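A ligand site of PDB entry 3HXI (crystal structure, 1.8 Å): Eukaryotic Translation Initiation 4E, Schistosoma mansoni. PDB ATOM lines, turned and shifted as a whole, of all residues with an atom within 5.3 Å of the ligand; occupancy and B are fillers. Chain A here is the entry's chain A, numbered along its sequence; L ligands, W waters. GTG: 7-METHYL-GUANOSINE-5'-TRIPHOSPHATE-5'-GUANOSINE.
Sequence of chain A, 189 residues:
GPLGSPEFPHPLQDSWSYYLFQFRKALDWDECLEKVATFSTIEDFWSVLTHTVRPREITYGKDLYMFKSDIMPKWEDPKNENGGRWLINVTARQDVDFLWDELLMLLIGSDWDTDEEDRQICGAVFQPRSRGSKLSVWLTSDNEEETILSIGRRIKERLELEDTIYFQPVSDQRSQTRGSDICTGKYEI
O6A of the ligand lies within hydrogen-bond range of N of Trp 75, at 2.8 Å. O1B of the ligand is in salt-bridge range of NE of Arg 129. O2G of the ligand lies within salt-bridge range of NE of Arg 178 (2.8 Å). An oxygen (O1B) of the ligand lies within salt-bridge range of the side-chain amino group (NZ) of Lys 134 (2.8 Å). The side-chain carboxylate of Glu 76 sits at hydrogen-bond distance from a nitrogen (N1A) of the ligand, 2.9 Å away. A nitrogen (N2B) of the ligand sits at hydrogen-bond distance from the backbone carbonyl oxygen (O) of Leu 27, at 3.1 Å. O of Gly 61 lies within hydrogen-bond range of O3E of the ligand (3.1 Å). O4D of the ligand sits close to NE1 of Trp 29 (3.3 Å). NE2 of Gln 127 lies within hydrogen-bond range of O2A of the ligand, 3.2 Å away.
OE1 of Gln 173 lies within hydrogen-bond range of NE1 of Trp 75, 2.9 Å away. The guanidinium group of Arg 129 sits close to the side-chain amide nitrogen of Gln 127. The guanidinium group (NH2) of Arg 129 is in salt-bridge range of the side-chain carboxylate (OD1) of Asp 63, at 2.8 Å. O of Lys 134 lies within hydrogen-bond range of N of Gln 127 (2.8 Å). The side-chain carboxylate (OE2) of Glu 76 is in salt-bridge range of the guanidinium group (NH2) of Arg 174 (3.0 Å). The side-chain amide nitrogen (NE2) of Gln 127 lies within hydrogen-bond range of the side-chain carboxylate (OD2) of Asp 63 (3.3 Å). The backbone NH (N) of Phe 21 is in hydrogen-bond range of the backbone carbonyl oxygen (O) of Asp 63. The backbone carbonyl oxygen (O) of Asp 28 is in hydrogen-bond range of the side-chain sulfur (SG) of Cys 32.
Phe 21 touches the ligand (CE2 to O4E, 3.5 Å). CB of Phe 23 touches O3E of the ligand (3.4 Å). Asp 28 touches the ligand. Cys 32 touches the ligand (SG to N2B, 3.8 Å). Tyr 65 touches the ligand (OH to C7X, 3.9 Å). Lys 74 touches the ligand. Trp 138 touches the ligand (CZ2 to C7X, 3.8 Å). Within 4 Å of the ligand: Phe 21, Phe 23, Leu 27, Asp 28, Trp 29, Cys 32, Gly 61, Tyr 65, Lys 74, Trp 75, Glu 76, Gln 127, Arg 129, Lys 134, Trp 138 and Arg 178. The nearest printed residue that does not touch the ligand is Asp 63 (4.3 Å).
Water W1 bridges an oxygen (O1A) of the ligand (2.6 Å) and the indole nitrogen (NE1) of Trp 29 (2.9 Å). Water W4 lies within hydrogen-bond range of the side-chain amide oxygen (OE1) of Gln 127, an oxygen (O2A) of the ligand, the guanidinium group (NH2) of Arg 85 and the side-chain amino group (NZ) of Lys 134. Water W6 bridges an oxygen (O3D) of the ligand (2.8 Å) and the backbone carbonyl oxygen (O) of Gln 176 (2.9 Å). Water W2 lies within hydrogen-bond range of a nitrogen (N1B) of the ligand and the backbone NH (N) of Trp 29. Water W8 lies within hydrogen-bond range of O of Gln 173 (2.8 Å) and O3D of the ligand (3.4 Å).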
ATOM      1  N   PHE A  21       6.877  -4.734  15.635  1.00  0.00           N
ATOM      2  CA  PHE A  21       6.299  -5.130  14.352  1.00  0.00           C
ATOM      3  C   PHE A  21       4.774  -5.160  14.487  1.00  0.00           C
ATOM      4  O   PHE A  21       4.239  -5.949  15.241  1.00  0.00           O
ATOM      5  CB  PHE A  21       6.814  -6.525  13.918  1.00  0.00           C
ATOM      6  CG  PHE A  21       6.179  -7.002  12.647  1.00  0.00           C
ATOM      7  CD1 PHE A  21       6.774  -6.738  11.416  1.00  0.00           C
ATOM      8  CD2 PHE A  21       4.953  -7.656  12.666  1.00  0.00           C
ATOM      9  CE1 PHE A  21       6.171  -7.143  10.233  1.00  0.00           C
ATOM     10  CE2 PHE A  21       4.355  -8.081  11.491  1.00  0.00           C
ATOM     11  CZ  PHE A  21       4.951  -7.803  10.266  1.00  0.00           C
ATOM     12  N   PHE A  23       1.382  -5.502  12.064  1.00  0.00           N
ATOM     13  CA  PHE A  23       0.865  -5.677  10.711  1.00  0.00           C
ATOM     14  C   PHE A  23      -0.333  -4.775  10.464  1.00  0.00           C
ATOM     15  O   PHE A  23      -1.277  -4.754  11.257  1.00  0.00           O
ATOM     16  CB  PHE A  23       0.468  -7.123  10.388  1.00  0.00           C
ATOM     17  CG  PHE A  23      -0.447  -7.240   9.185  1.00  0.00           C
ATOM     18  CD1 PHE A  23       0.081  -7.139   7.892  1.00  0.00           C
ATOM     19  CD2 PHE A  23      -1.814  -7.428   9.351  1.00  0.00           C
ATOM     20  CE1 PHE A  23      -0.752  -7.222   6.773  1.00  0.00           C
ATOM     21  CE2 PHE A  23      -2.653  -7.515   8.239  1.00  0.00           C
ATOM     22  CZ  PHE A  23      -2.113  -7.407   6.946  1.00  0.00           C
ATOM     23  N   ARG A  24      -0.271  -4.031   9.362  1.00  0.00           N
ATOM     24  CA  ARG A  24      -1.454  -3.399   8.798  1.00  0.00           C
ATOM     25  C   ARG A  24      -1.511  -3.733   7.317  1.00  0.00           C
ATOM     26  O   ARG A  24      -0.456  -3.899   6.661  1.00  0.00           O
ATOM     27  CB  ARG A  24      -1.462  -1.880   9.037  1.00  0.00           C
ATOM     28  CG  ARG A  24      -1.701  -1.483  10.506  1.00  0.00           C
ATOM     29  CD  ARG A  24      -0.387  -1.337  11.270  1.00  0.00           C
ATOM     30  NE  ARG A  24       0.277  -0.075  10.934  1.00  0.00           N
ATOM     31  CZ  ARG A  24       1.586   0.157  11.069  1.00  0.00           C
ATOM     32  NH1 ARG A  24       2.061   1.348  10.722  1.00  0.00           N
ATOM     33  NH2 ARG A  24       2.421  -0.767  11.543  1.00  0.00           N
ATOM     34  N   LEU A  27       0.771  -2.738   3.783  1.00  0.00           N
ATOM     35  CA  LEU A  27       2.137  -2.283   4.083  1.00  0.00           C
ATOM     36  C   LEU A  27       3.101  -3.415   3.769  1.00  0.00           C
ATOM     37  O   LEU A  27       2.785  -4.585   4.010  1.00  0.00           O
ATOM     38  CB  LEU A  27       2.265  -1.849   5.544  1.00  0.00           C
ATOM     39  CG  LEU A  27       1.576  -0.551   5.969  1.00  0.00           C
ATOM     40  CD1 LEU A  27       1.698  -0.387   7.483  1.00  0.00           C
ATOM     41  CD2 LEU A  27       2.155   0.669   5.253  1.00  0.00           C
ATOM     42  N   ASP A  28       4.273  -3.077   3.231  1.00  0.00           N
ATOM     43  CA  ASP A  28       5.336  -4.069   3.037  1.00  0.00           C
ATOM     44  C   ASP A  28       5.792  -4.532   4.422  1.00  0.00           C
ATOM     45  O   ASP A  28       5.595  -3.811   5.410  1.00  0.00           O
ATOM     46  CB  ASP A  28       6.514  -3.471   2.263  1.00  0.00           C
ATOM     47  CG  ASP A  28       6.166  -3.159   0.804  1.00  0.00           C
ATOM     48  OD1 ASP A  28       5.157  -3.666   0.283  1.00  0.00           O
ATOM     49  OD2 ASP A  28       6.913  -2.395   0.173  1.00  0.00           O
ATOM     50  N   TRP A  29       6.391  -5.712   4.485  1.00  0.00           N
ATOM     51  CA  TRP A  29       6.848  -6.263   5.761  1.00  0.00           C
ATOM     52  C   TRP A  29       7.693  -5.262   6.562  1.00  0.00           C
ATOM     53  O   TRP A  29       7.441  -5.022   7.743  1.00  0.00           O
ATOM     54  CB  TRP A  29       7.595  -7.604   5.573  1.00  0.00           C
ATOM     55  CG  TRP A  29       7.989  -8.239   6.897  1.00  0.00           C
ATOM     56  CD1 TRP A  29       7.251  -9.119   7.634  1.00  0.00           C
ATOM     57  CD2 TRP A  29       9.210  -8.024   7.614  1.00  0.00           C
ATOM     58  NE1 TRP A  29       7.947  -9.472   8.787  1.00  0.00           N
ATOM     59  CE2 TRP A  29       9.145  -8.799   8.795  1.00  0.00           C
ATOM     60  CE3 TRP A  29      10.352  -7.248   7.375  1.00  0.00           C
ATOM     61  CZ2 TRP A  29      10.188  -8.809   9.745  1.00  0.00           C
ATOM     62  CZ3 TRP A  29      11.383  -7.266   8.310  1.00  0.00           C
ATOM     63  CH2 TRP A  29      11.289  -8.048   9.478  1.00  0.00           C
ATOM     64  N   CYS A  32       6.092  -2.360   8.441  1.00  0.00           N
ATOM     65  CA  CYS A  32       5.332  -2.681   9.646  1.00  0.00           C
ATOM     66  C   CYS A  32       6.176  -2.581  10.906  1.00  0.00           C
ATOM     67  O   CYS A  32       5.640  -2.652  12.012  1.00  0.00           O
ATOM     68  CB  CYS A  32       4.715  -4.083   9.559  1.00  0.00           C
ATOM     69  SG  CYS A  32       3.464  -4.332   8.263  1.00  0.00           S
ATOM     70  N   GLY A  61       0.781 -12.060  16.761  1.00  0.00           N
ATOM     71  CA  GLY A  61       1.294 -11.530  15.498  1.00  0.00           C
ATOM     72  C   GLY A  61       1.972 -10.161  15.580  1.00  0.00           C
ATOM     73  O   GLY A  61       2.453  -9.660  14.553  1.00  0.00           O
ATOM     74  N   LYS A  62       1.968  -9.555  16.775  1.00  0.00           N
ATOM     75  CA  LYS A  62       2.691  -8.288  17.041  1.00  0.00           C
ATOM     76  C   LYS A  62       4.004  -8.655  17.710  1.00  0.00           C
ATOM     77  O   LYS A  62       3.995  -9.299  18.749  1.00  0.00           O
ATOM     78  CB  LYS A  62       1.887  -7.370  17.957  1.00  0.00           C
ATOM     79  CG  LYS A  62       2.701  -6.158  18.496  1.00  0.00           C
ATOM     80  CD  LYS A  62       1.813  -5.141  19.221  1.00  0.00           C
ATOM     81  CE  LYS A  62       2.609  -4.343  20.260  1.00  0.00           C
ATOM     82  NZ  LYS A  62       1.883  -3.092  20.674  1.00  0.00           N
ATOM     83  N   ASP A  63       5.114  -8.290  17.092  1.00  0.00           N
ATOM     84  CA  ASP A  63       6.395  -8.836  17.488  1.00  0.00           C
ATOM     85  C   ASP A  63       7.311  -7.758  18.064  1.00  0.00           C
ATOM     86  O   ASP A  63       7.143  -6.574  17.770  1.00  0.00           O
ATOM     87  CB  ASP A  63       7.076  -9.541  16.303  1.00  0.00           C
ATOM     88  CG  ASP A  63       6.247 -10.705  15.733  1.00  0.00           C
ATOM     89  OD1 ASP A  63       5.295 -11.134  16.398  1.00  0.00           O
ATOM     90  OD2 ASP A  63       6.557 -11.211  14.618  1.00  0.00           O
ATOM     91  N   TYR A  65      11.426  -6.697  18.506  1.00  0.00           N
ATOM     92  CA  TYR A  65      12.785  -6.891  17.966  1.00  0.00           C
ATOM     93  C   TYR A  65      13.755  -6.025  18.755  1.00  0.00           C
ATOM     94  O   TYR A  65      13.515  -4.810  18.883  1.00  0.00           O
ATOM     95  CB  TYR A  65      12.849  -6.466  16.488  1.00  0.00           C
ATOM     96  CG  TYR A  65      12.221  -7.439  15.496  1.00  0.00           C
ATOM     97  CD1 TYR A  65      13.036  -8.249  14.680  1.00  0.00           C
ATOM     98  CD2 TYR A  65      10.815  -7.553  15.374  1.00  0.00           C
ATOM     99  CE1 TYR A  65      12.469  -9.155  13.769  1.00  0.00           C
ATOM    100  CE2 TYR A  65      10.249  -8.447  14.469  1.00  0.00           C
ATOM    101  CZ  TYR A  65      11.076  -9.248  13.667  1.00  0.00           C
ATOM    102  OH  TYR A  65      10.550 -10.164  12.771  1.00  0.00           O
ATOM    103  N   PRO A  73      16.689  -4.566  11.852  1.00  0.00           N
ATOM    104  CA  PRO A  73      16.115  -5.865  12.206  1.00  0.00           C
ATOM    105  C   PRO A  73      15.454  -6.566  11.019  1.00  0.00           C
ATOM    106  O   PRO A  73      14.247  -6.807  11.020  1.00  0.00           O
ATOM    107  CB  PRO A  73      15.057  -5.485  13.260  1.00  0.00           C
ATOM    108  CG  PRO A  73      14.599  -4.147  12.834  1.00  0.00           C
ATOM    109  CD  PRO A  73      15.816  -3.441  12.280  1.00  0.00           C
ATOM    110  N   LYS A  74      16.242  -6.898   9.996  1.00  0.00           N
ATOM    111  CA  LYS A  74      15.703  -7.581   8.824  1.00  0.00           C
ATOM    112  C   LYS A  74      16.810  -8.332   8.112  1.00  0.00           C
ATOM    113  O   LYS A  74      17.992  -7.989   8.275  1.00  0.00           O
ATOM    114  CB  LYS A  74      14.962  -6.606   7.887  1.00  0.00           C
ATOM    115  CG  LYS A  74      15.825  -5.549   7.211  1.00  0.00           C
ATOM    116  CD  LYS A  74      14.989  -4.359   6.678  1.00  0.00           C
ATOM    117  CE  LYS A  74      14.356  -4.618   5.302  1.00  0.00           C
ATOM    118  NZ  LYS A  74      14.147  -3.337   4.534  1.00  0.00           N
ATOM    119  N   TRP A  75      16.437  -9.356   7.352  1.00  0.00           N
ATOM    120  CA  TRP A  75      17.419 -10.237   6.739  1.00  0.00           C
ATOM    121  C   TRP A  75      18.344  -9.440   5.831  1.00  0.00           C
ATOM    122  O   TRP A  75      19.529  -9.777   5.661  1.00  0.00           O
ATOM    123  CB  TRP A  75      16.743 -11.314   5.881  1.00  0.00           C
ATOM    124  CG  TRP A  75      15.877 -12.308   6.639  1.00  0.00           C
ATOM    125  CD1 TRP A  75      16.148 -12.898   7.839  1.00  0.00           C
ATOM    126  CD2 TRP A  75      14.629 -12.841   6.196  1.00  0.00           C
ATOM    127  NE1 TRP A  75      15.115 -13.739   8.196  1.00  0.00           N
ATOM    128  CE2 TRP A  75      14.177 -13.739   7.192  1.00  0.00           C
ATOM    129  CE3 TRP A  75      13.858 -12.664   5.040  1.00  0.00           C
ATOM    130  CZ2 TRP A  75      12.989 -14.448   7.080  1.00  0.00           C
ATOM    131  CZ3 TRP A  75      12.665 -13.377   4.921  1.00  0.00           C
ATOM    132  CH2 TRP A  75      12.237 -14.259   5.930  1.00  0.00           C
ATOM    133  N   GLU A  76      17.784  -8.375   5.266  1.00  0.00           N
ATOM    134  CA  GLU A  76      18.473  -7.592   4.222  1.00  0.00           C
ATOM    135  C   GLU A  76      19.729  -6.830   4.679  1.00  0.00           C
ATOM    136  O   GLU A  76      20.581  -6.463   3.832  1.00  0.00           O
ATOM    137  CB  GLU A  76      17.465  -6.673   3.507  1.00  0.00           C
ATOM    138  CG  GLU A  76      16.468  -7.433   2.620  1.00  0.00           C
ATOM    139  CD  GLU A  76      15.362  -8.187   3.383  1.00  0.00           C
ATOM    140  OE1 GLU A  76      15.036  -7.829   4.542  1.00  0.00           O
ATOM    141  OE2 GLU A  76      14.828  -9.156   2.816  1.00  0.00           O
ATOM    142  N   ARG A  85      19.505 -17.745  12.851  1.00  0.00           N
ATOM    143  CA  ARG A  85      18.914 -17.541  14.173  1.00  0.00           C
ATOM    144  C   ARG A  85      18.852 -18.824  14.975  1.00  0.00           C
ATOM    145  O   ARG A  85      18.607 -19.896  14.424  1.00  0.00           O
ATOM    146  CB  ARG A  85      17.495 -16.933  14.049  1.00  0.00           C
ATOM    147  CG  ARG A  85      16.455 -17.939  13.581  1.00  0.00           C
ATOM    148  CD  ARG A  85      15.101 -17.306  13.398  1.00  0.00           C
ATOM    149  NE  ARG A  85      14.161 -18.298  12.923  1.00  0.00           N
ATOM    150  CZ  ARG A  85      12.841 -18.132  12.834  1.00  0.00           C
ATOM    151  NH1 ARG A  85      12.095 -19.154  12.396  1.00  0.00           N
ATOM    152  NH2 ARG A  85      12.283 -16.984  13.163  1.00  0.00           N
ATOM    153  N   GLN A 127       8.038 -13.410  19.178  1.00  0.00           N
ATOM    154  CA  GLN A 127       6.905 -13.548  18.265  1.00  0.00           C
ATOM    155  C   GLN A 127       5.775 -14.335  18.938  1.00  0.00           C
ATOM    156  O   GLN A 127       5.821 -15.563  19.000  1.00  0.00           O
ATOM    157  CB  GLN A 127       7.341 -14.212  16.963  1.00  0.00           C
ATOM    158  CG  GLN A 127       8.430 -13.443  16.235  1.00  0.00           C
ATOM    159  CD  GLN A 127       8.907 -14.171  15.008  1.00  0.00           C
ATOM    160  OE1 GLN A 127       9.441 -15.272  15.093  1.00  0.00           O
ATOM    161  NE2 GLN A 127       8.702 -13.550  13.848  1.00  0.00           N
ATOM    162  N   ARG A 129       2.400 -16.175  19.024  1.00  0.00           N
ATOM    163  CA  ARG A 129       1.560 -16.832  18.039  1.00  0.00           C
ATOM    164  C   ARG A 129       0.594 -17.762  18.743  1.00  0.00           C
ATOM    165  O   ARG A 129       0.923 -18.362  19.767  1.00  0.00           O
ATOM    166  CB  ARG A 129       2.387 -17.656  17.061  1.00  0.00           C
ATOM    167  CG  ARG A 129       3.419 -16.894  16.227  1.00  0.00           C
ATOM    168  CD  ARG A 129       2.762 -15.991  15.189  1.00  0.00           C
ATOM    169  NE  ARG A 129       3.788 -15.325  14.389  1.00  0.00           N
ATOM    170  CZ  ARG A 129       4.412 -14.219  14.749  1.00  0.00           C
ATOM    171  NH1 ARG A 129       5.332 -13.689  13.950  1.00  0.00           N
ATOM    172  NH2 ARG A 129       4.102 -13.617  15.893  1.00  0.00           N
ATOM    173  N   LYS A 134       7.425 -17.907  19.665  1.00  0.00           N
ATOM    174  CA  LYS A 134       8.801 -18.174  19.301  1.00  0.00           C
ATOM    175  C   LYS A 134       9.679 -17.051  19.839  1.00  0.00           C
ATOM    176  O   LYS A 134       9.300 -15.877  19.764  1.00  0.00           O
ATOM    177  CB  LYS A 134       8.950 -18.252  17.790  1.00  0.00           C
ATOM    178  CG  LYS A 134       8.174 -19.413  17.128  1.00  0.00           C
ATOM    179  CD  LYS A 134       8.248 -19.301  15.627  1.00  0.00           C
ATOM    180  CE  LYS A 134       7.248 -18.236  15.094  1.00  0.00           C
ATOM    181  NZ  LYS A 134       7.032 -18.407  13.622  1.00  0.00           N
ATOM    182  N   TRP A 138      19.326 -13.708  16.609  1.00  0.00           N
ATOM    183  CA  TRP A 138      19.923 -13.613  15.289  1.00  0.00           C
ATOM    184  C   TRP A 138      21.421 -13.393  15.426  1.00  0.00           C
ATOM    185  O   TRP A 138      21.848 -12.534  16.226  1.00  0.00           O
ATOM    186  CB  TRP A 138      19.297 -12.409  14.580  1.00  0.00           C
ATOM    187  CG  TRP A 138      17.894 -12.641  14.075  1.00  0.00           C
ATOM    188  CD1 TRP A 138      16.904 -13.431  14.629  1.00  0.00           C
ATOM    189  CD2 TRP A 138      17.312 -12.029  12.915  1.00  0.00           C
ATOM    190  NE1 TRP A 138      15.748 -13.337  13.872  1.00  0.00           N
ATOM    191  CE2 TRP A 138      15.984 -12.495  12.808  1.00  0.00           C
ATOM    192  CE3 TRP A 138      17.805 -11.127  11.955  1.00  0.00           C
ATOM    193  CZ2 TRP A 138      15.133 -12.102  11.765  1.00  0.00           C
ATOM    194  CZ3 TRP A 138      16.959 -10.741  10.927  1.00  0.00           C
ATOM    195  CH2 TRP A 138      15.630 -11.218  10.842  1.00  0.00           C
ATOM    196  N   GLN A 173      15.258 -19.574   6.477  1.00  0.00           N
ATOM    197  CA  GLN A 173      14.173 -18.696   6.947  1.00  0.00           C
ATOM    198  C   GLN A 173      13.411 -18.103   5.765  1.00  0.00           C
ATOM    199  O   GLN A 173      12.180 -18.090   5.749  1.00  0.00           O
ATOM    200  CB  GLN A 173      14.724 -17.577   7.830  1.00  0.00           C
ATOM    201  CG  GLN A 173      15.325 -18.023   9.165  1.00  0.00           C
ATOM    202  CD  GLN A 173      15.897 -16.862   9.961  1.00  0.00           C
ATOM    203  OE1 GLN A 173      15.245 -15.851  10.149  1.00  0.00           O
ATOM    204  NE2 GLN A 173      17.134 -16.997  10.395  1.00  0.00           N
ATOM    205  N   ARG A 174      14.133 -17.615   4.768  1.00  0.00           N
ATOM    206  CA  ARG A 174      13.538 -17.038   3.567  1.00  0.00           C
ATOM    207  C   ARG A 174      12.578 -17.996   2.883  1.00  0.00           C
ATOM    208  O   ARG A 174      11.490 -17.605   2.427  1.00  0.00           O
ATOM    209  CB  ARG A 174      14.620 -16.621   2.563  1.00  0.00           C
ATOM    210  CG  ARG A 174      15.533 -15.516   3.052  1.00  0.00           C
ATOM    211  CD  ARG A 174      16.463 -15.061   1.925  1.00  0.00           C
ATOM    212  NE  ARG A 174      16.920 -13.692   2.112  1.00  0.00           N
ATOM    213  CZ  ARG A 174      16.142 -12.616   1.976  1.00  0.00           C
ATOM    214  NH1 ARG A 174      14.865 -12.746   1.651  1.00  0.00           N
ATOM    215  NH2 ARG A 174      16.648 -11.406   2.160  1.00  0.00           N
ATOM    216  N   GLN A 176      11.094 -20.710   4.113  1.00  0.00           N
ATOM    217  CA  GLN A 176      10.100 -21.316   4.994  1.00  0.00           C
ATOM    218  C   GLN A 176       8.675 -20.830   4.686  1.00  0.00           C
ATOM    219  O   GLN A 176       8.442 -19.642   4.505  1.00  0.00           O
ATOM    220  CB  GLN A 176      10.423 -20.996   6.457  1.00  0.00           C
ATOM    221  CG  GLN A 176       9.850 -21.969   7.456  1.00  0.00           C
ATOM    222  CD  GLN A 176      10.684 -22.041   8.713  1.00  0.00           C
ATOM    223  OE1 GLN A 176      11.221 -21.028   9.192  1.00  0.00           O
ATOM    224  NE2 GLN A 176      10.801 -23.251   9.270  1.00  0.00           N
ATOM    225  N   ARG A 178       4.854 -20.065   5.578  1.00  0.00           N
ATOM    226  CA  ARG A 178       3.986 -19.786   6.718  1.00  0.00           C
ATOM    227  C   ARG A 178       3.005 -20.963   6.855  1.00  0.00           C
ATOM    228  O   ARG A 178       2.460 -21.437   5.868  1.00  0.00           O
ATOM    229  CB  ARG A 178       3.247 -18.466   6.518  1.00  0.00           C
ATOM    230  CG  ARG A 178       4.162 -17.236   6.376  1.00  0.00           C
ATOM    231  CD  ARG A 178       3.418 -16.066   5.732  1.00  0.00           C
ATOM    232  NE  ARG A 178       2.280 -15.623   6.541  1.00  0.00           N
ATOM    233  CZ  ARG A 178       1.259 -14.895   6.086  1.00  0.00           C
ATOM    234  NH1 ARG A 178       1.218 -14.533   4.809  1.00  0.00           N
ATOM    235  NH2 ARG A 178       0.265 -14.551   6.901  1.00  0.00           N
ATOM    236  N   GLY A 179       2.841 -21.467   8.076  1.00  0.00           N
ATOM    237  CA  GLY A 179       1.931 -22.594   8.310  1.00  0.00           C
ATOM    238  C   GLY A 179       2.499 -24.012   8.267  1.00  0.00           C
ATOM    239  O   GLY A 179       1.825 -24.958   8.669  1.00  0.00           O
HETATM  240  PA  GTG L   1       7.349 -14.752  10.479  1.00  0.00           P
HETATM  241  O1A GTG L   1       6.439 -13.731  11.118  1.00  0.00           O
HETATM  242  O2A GTG L   1       8.737 -15.046  11.023  1.00  0.00           O
HETATM  243  O3A GTG L   1       6.617 -16.174  10.286  1.00  0.00           O
HETATM  244  PB  GTG L   1       5.265 -16.713  10.899  1.00  0.00           P
HETATM  245  O1B GTG L   1       5.241 -16.582  12.400  1.00  0.00           O
HETATM  246  O2B GTG L   1       5.055 -18.087  10.267  1.00  0.00           O
HETATM  247  O3B GTG L   1       4.210 -15.716  10.207  1.00  0.00           O
HETATM  248  N9A GTG L   1       9.670 -11.622   6.799  1.00  0.00           N
HETATM  249  C8A GTG L   1      10.068 -12.014   8.016  1.00  0.00           C
HETATM  250  N7A GTG L   1      11.289 -11.488   8.253  1.00  0.00           N
HETATM  251  C7X GTG L   1      12.056 -11.708   9.511  1.00  0.00           C
HETATM  252  C5A GTG L   1      11.649 -10.782   7.177  1.00  0.00           C
HETATM  253  C6A GTG L   1      12.796 -10.043   6.883  1.00  0.00           C
HETATM  254  O6A GTG L   1      13.761  -9.934   7.683  1.00  0.00           O
HETATM  255  N1A GTG L   1      12.879  -9.446   5.677  1.00  0.00           N
HETATM  256  C2A GTG L   1      11.829  -9.543   4.784  1.00  0.00           C
HETATM  257  N2A GTG L   1      11.883  -8.953   3.579  1.00  0.00           N
HETATM  258  N3A GTG L   1      10.713 -10.252   5.076  1.00  0.00           N
HETATM  259  C4A GTG L   1      10.624 -10.865   6.269  1.00  0.00           C
HETATM  260  O5D GTG L   1       7.566 -14.280   8.984  1.00  0.00           O
HETATM  261  C5D GTG L   1       6.418 -14.080   8.157  1.00  0.00           C
HETATM  262  C4D GTG L   1       6.865 -13.514   6.828  1.00  0.00           C
HETATM  263  O4D GTG L   1       7.359 -12.203   7.047  1.00  0.00           O
HETATM  264  C3D GTG L   1       8.000 -14.267   6.180  1.00  0.00           C
HETATM  265  O3D GTG L   1       7.521 -15.412   5.469  1.00  0.00           O
HETATM  266  C2D GTG L   1       8.588 -13.220   5.269  1.00  0.00           C
HETATM  267  O2D GTG L   1       7.808 -13.110   4.074  1.00  0.00           O
HETATM  268  C1D GTG L   1       8.402 -11.948   6.103  1.00  0.00           C
HETATM  269  PG  GTG L   1       2.643 -15.571  10.522  1.00  0.00           P
HETATM  270  O1G GTG L   1       2.262 -16.096  11.870  1.00  0.00           O
HETATM  271  O2G GTG L   1       1.863 -16.029   9.305  1.00  0.00           O
HETATM  272  O5E GTG L   1       2.537 -13.972  10.563  1.00  0.00           O
HETATM  273  C5E GTG L   1       3.079 -13.245  11.662  1.00  0.00           C
HETATM  274  C4E GTG L   1       2.766 -11.765  11.505  1.00  0.00           C
HETATM  275  O4E GTG L   1       3.420 -11.282  10.338  1.00  0.00           O
HETATM  276  C3E GTG L   1       1.292 -11.490  11.294  1.00  0.00           C
HETATM  277  O3E GTG L   1       1.032 -10.169  11.799  1.00  0.00           O
HETATM  278  C2E GTG L   1       1.118 -11.462   9.782  1.00  0.00           C
HETATM  279  O2E GTG L   1       0.002 -10.674   9.358  1.00  0.00           O
HETATM  280  C1E GTG L   1       2.445 -10.831   9.383  1.00  0.00           C
HETATM  281  N9B GTG L   1       2.982 -11.151   8.046  1.00  0.00           N
HETATM  282  C8B GTG L   1       3.246 -12.557   7.837  1.00  0.00           C
HETATM  283  N7B GTG L   1       3.804 -12.536   6.479  1.00  0.00           N
HETATM  284  C5B GTG L   1       3.859 -11.233   6.066  1.00  0.00           C
HETATM  285  C6B GTG L   1       4.315 -10.583   4.824  1.00  0.00           C
HETATM  286  O6B GTG L   1       4.777 -11.324   3.909  1.00  0.00           O
HETATM  287  N1B GTG L   1       4.202  -9.235   4.718  1.00  0.00           N
HETATM  288  C2B GTG L   1       3.689  -8.460   5.744  1.00  0.00           C
HETATM  289  N2B GTG L   1       3.593  -7.113   5.624  1.00  0.00           N
HETATM  290  N3B GTG L   1       3.252  -8.996   6.915  1.00  0.00           N
HETATM  291  C4B GTG L   1       3.325 -10.329   7.104  1.00  0.00           C
HETATM  292  O   HOH W   1       6.422 -11.132  10.652  1.00  0.00           O
HETATM  293  O   HOH W   2       4.957  -7.737   2.455  1.00  0.00           O
HETATM  294  O   HOH W   3       7.087 -19.333   8.905  1.00  0.00           O
HETATM  295  O   HOH W   4       9.423 -16.876  12.919  1.00  0.00           O
HETATM  296  O   HOH W   5       2.308 -18.664  13.064  1.00  0.00           O
HETATM  297  O   HOH W   6       7.634 -17.912   6.709  1.00  0.00           O
HETATM  298  O   HOH W   7      10.733 -15.953   9.589  1.00  0.00           O
HETATM  299  O   HOH W   8      10.013 -16.977   7.091  1.00  0.00           O
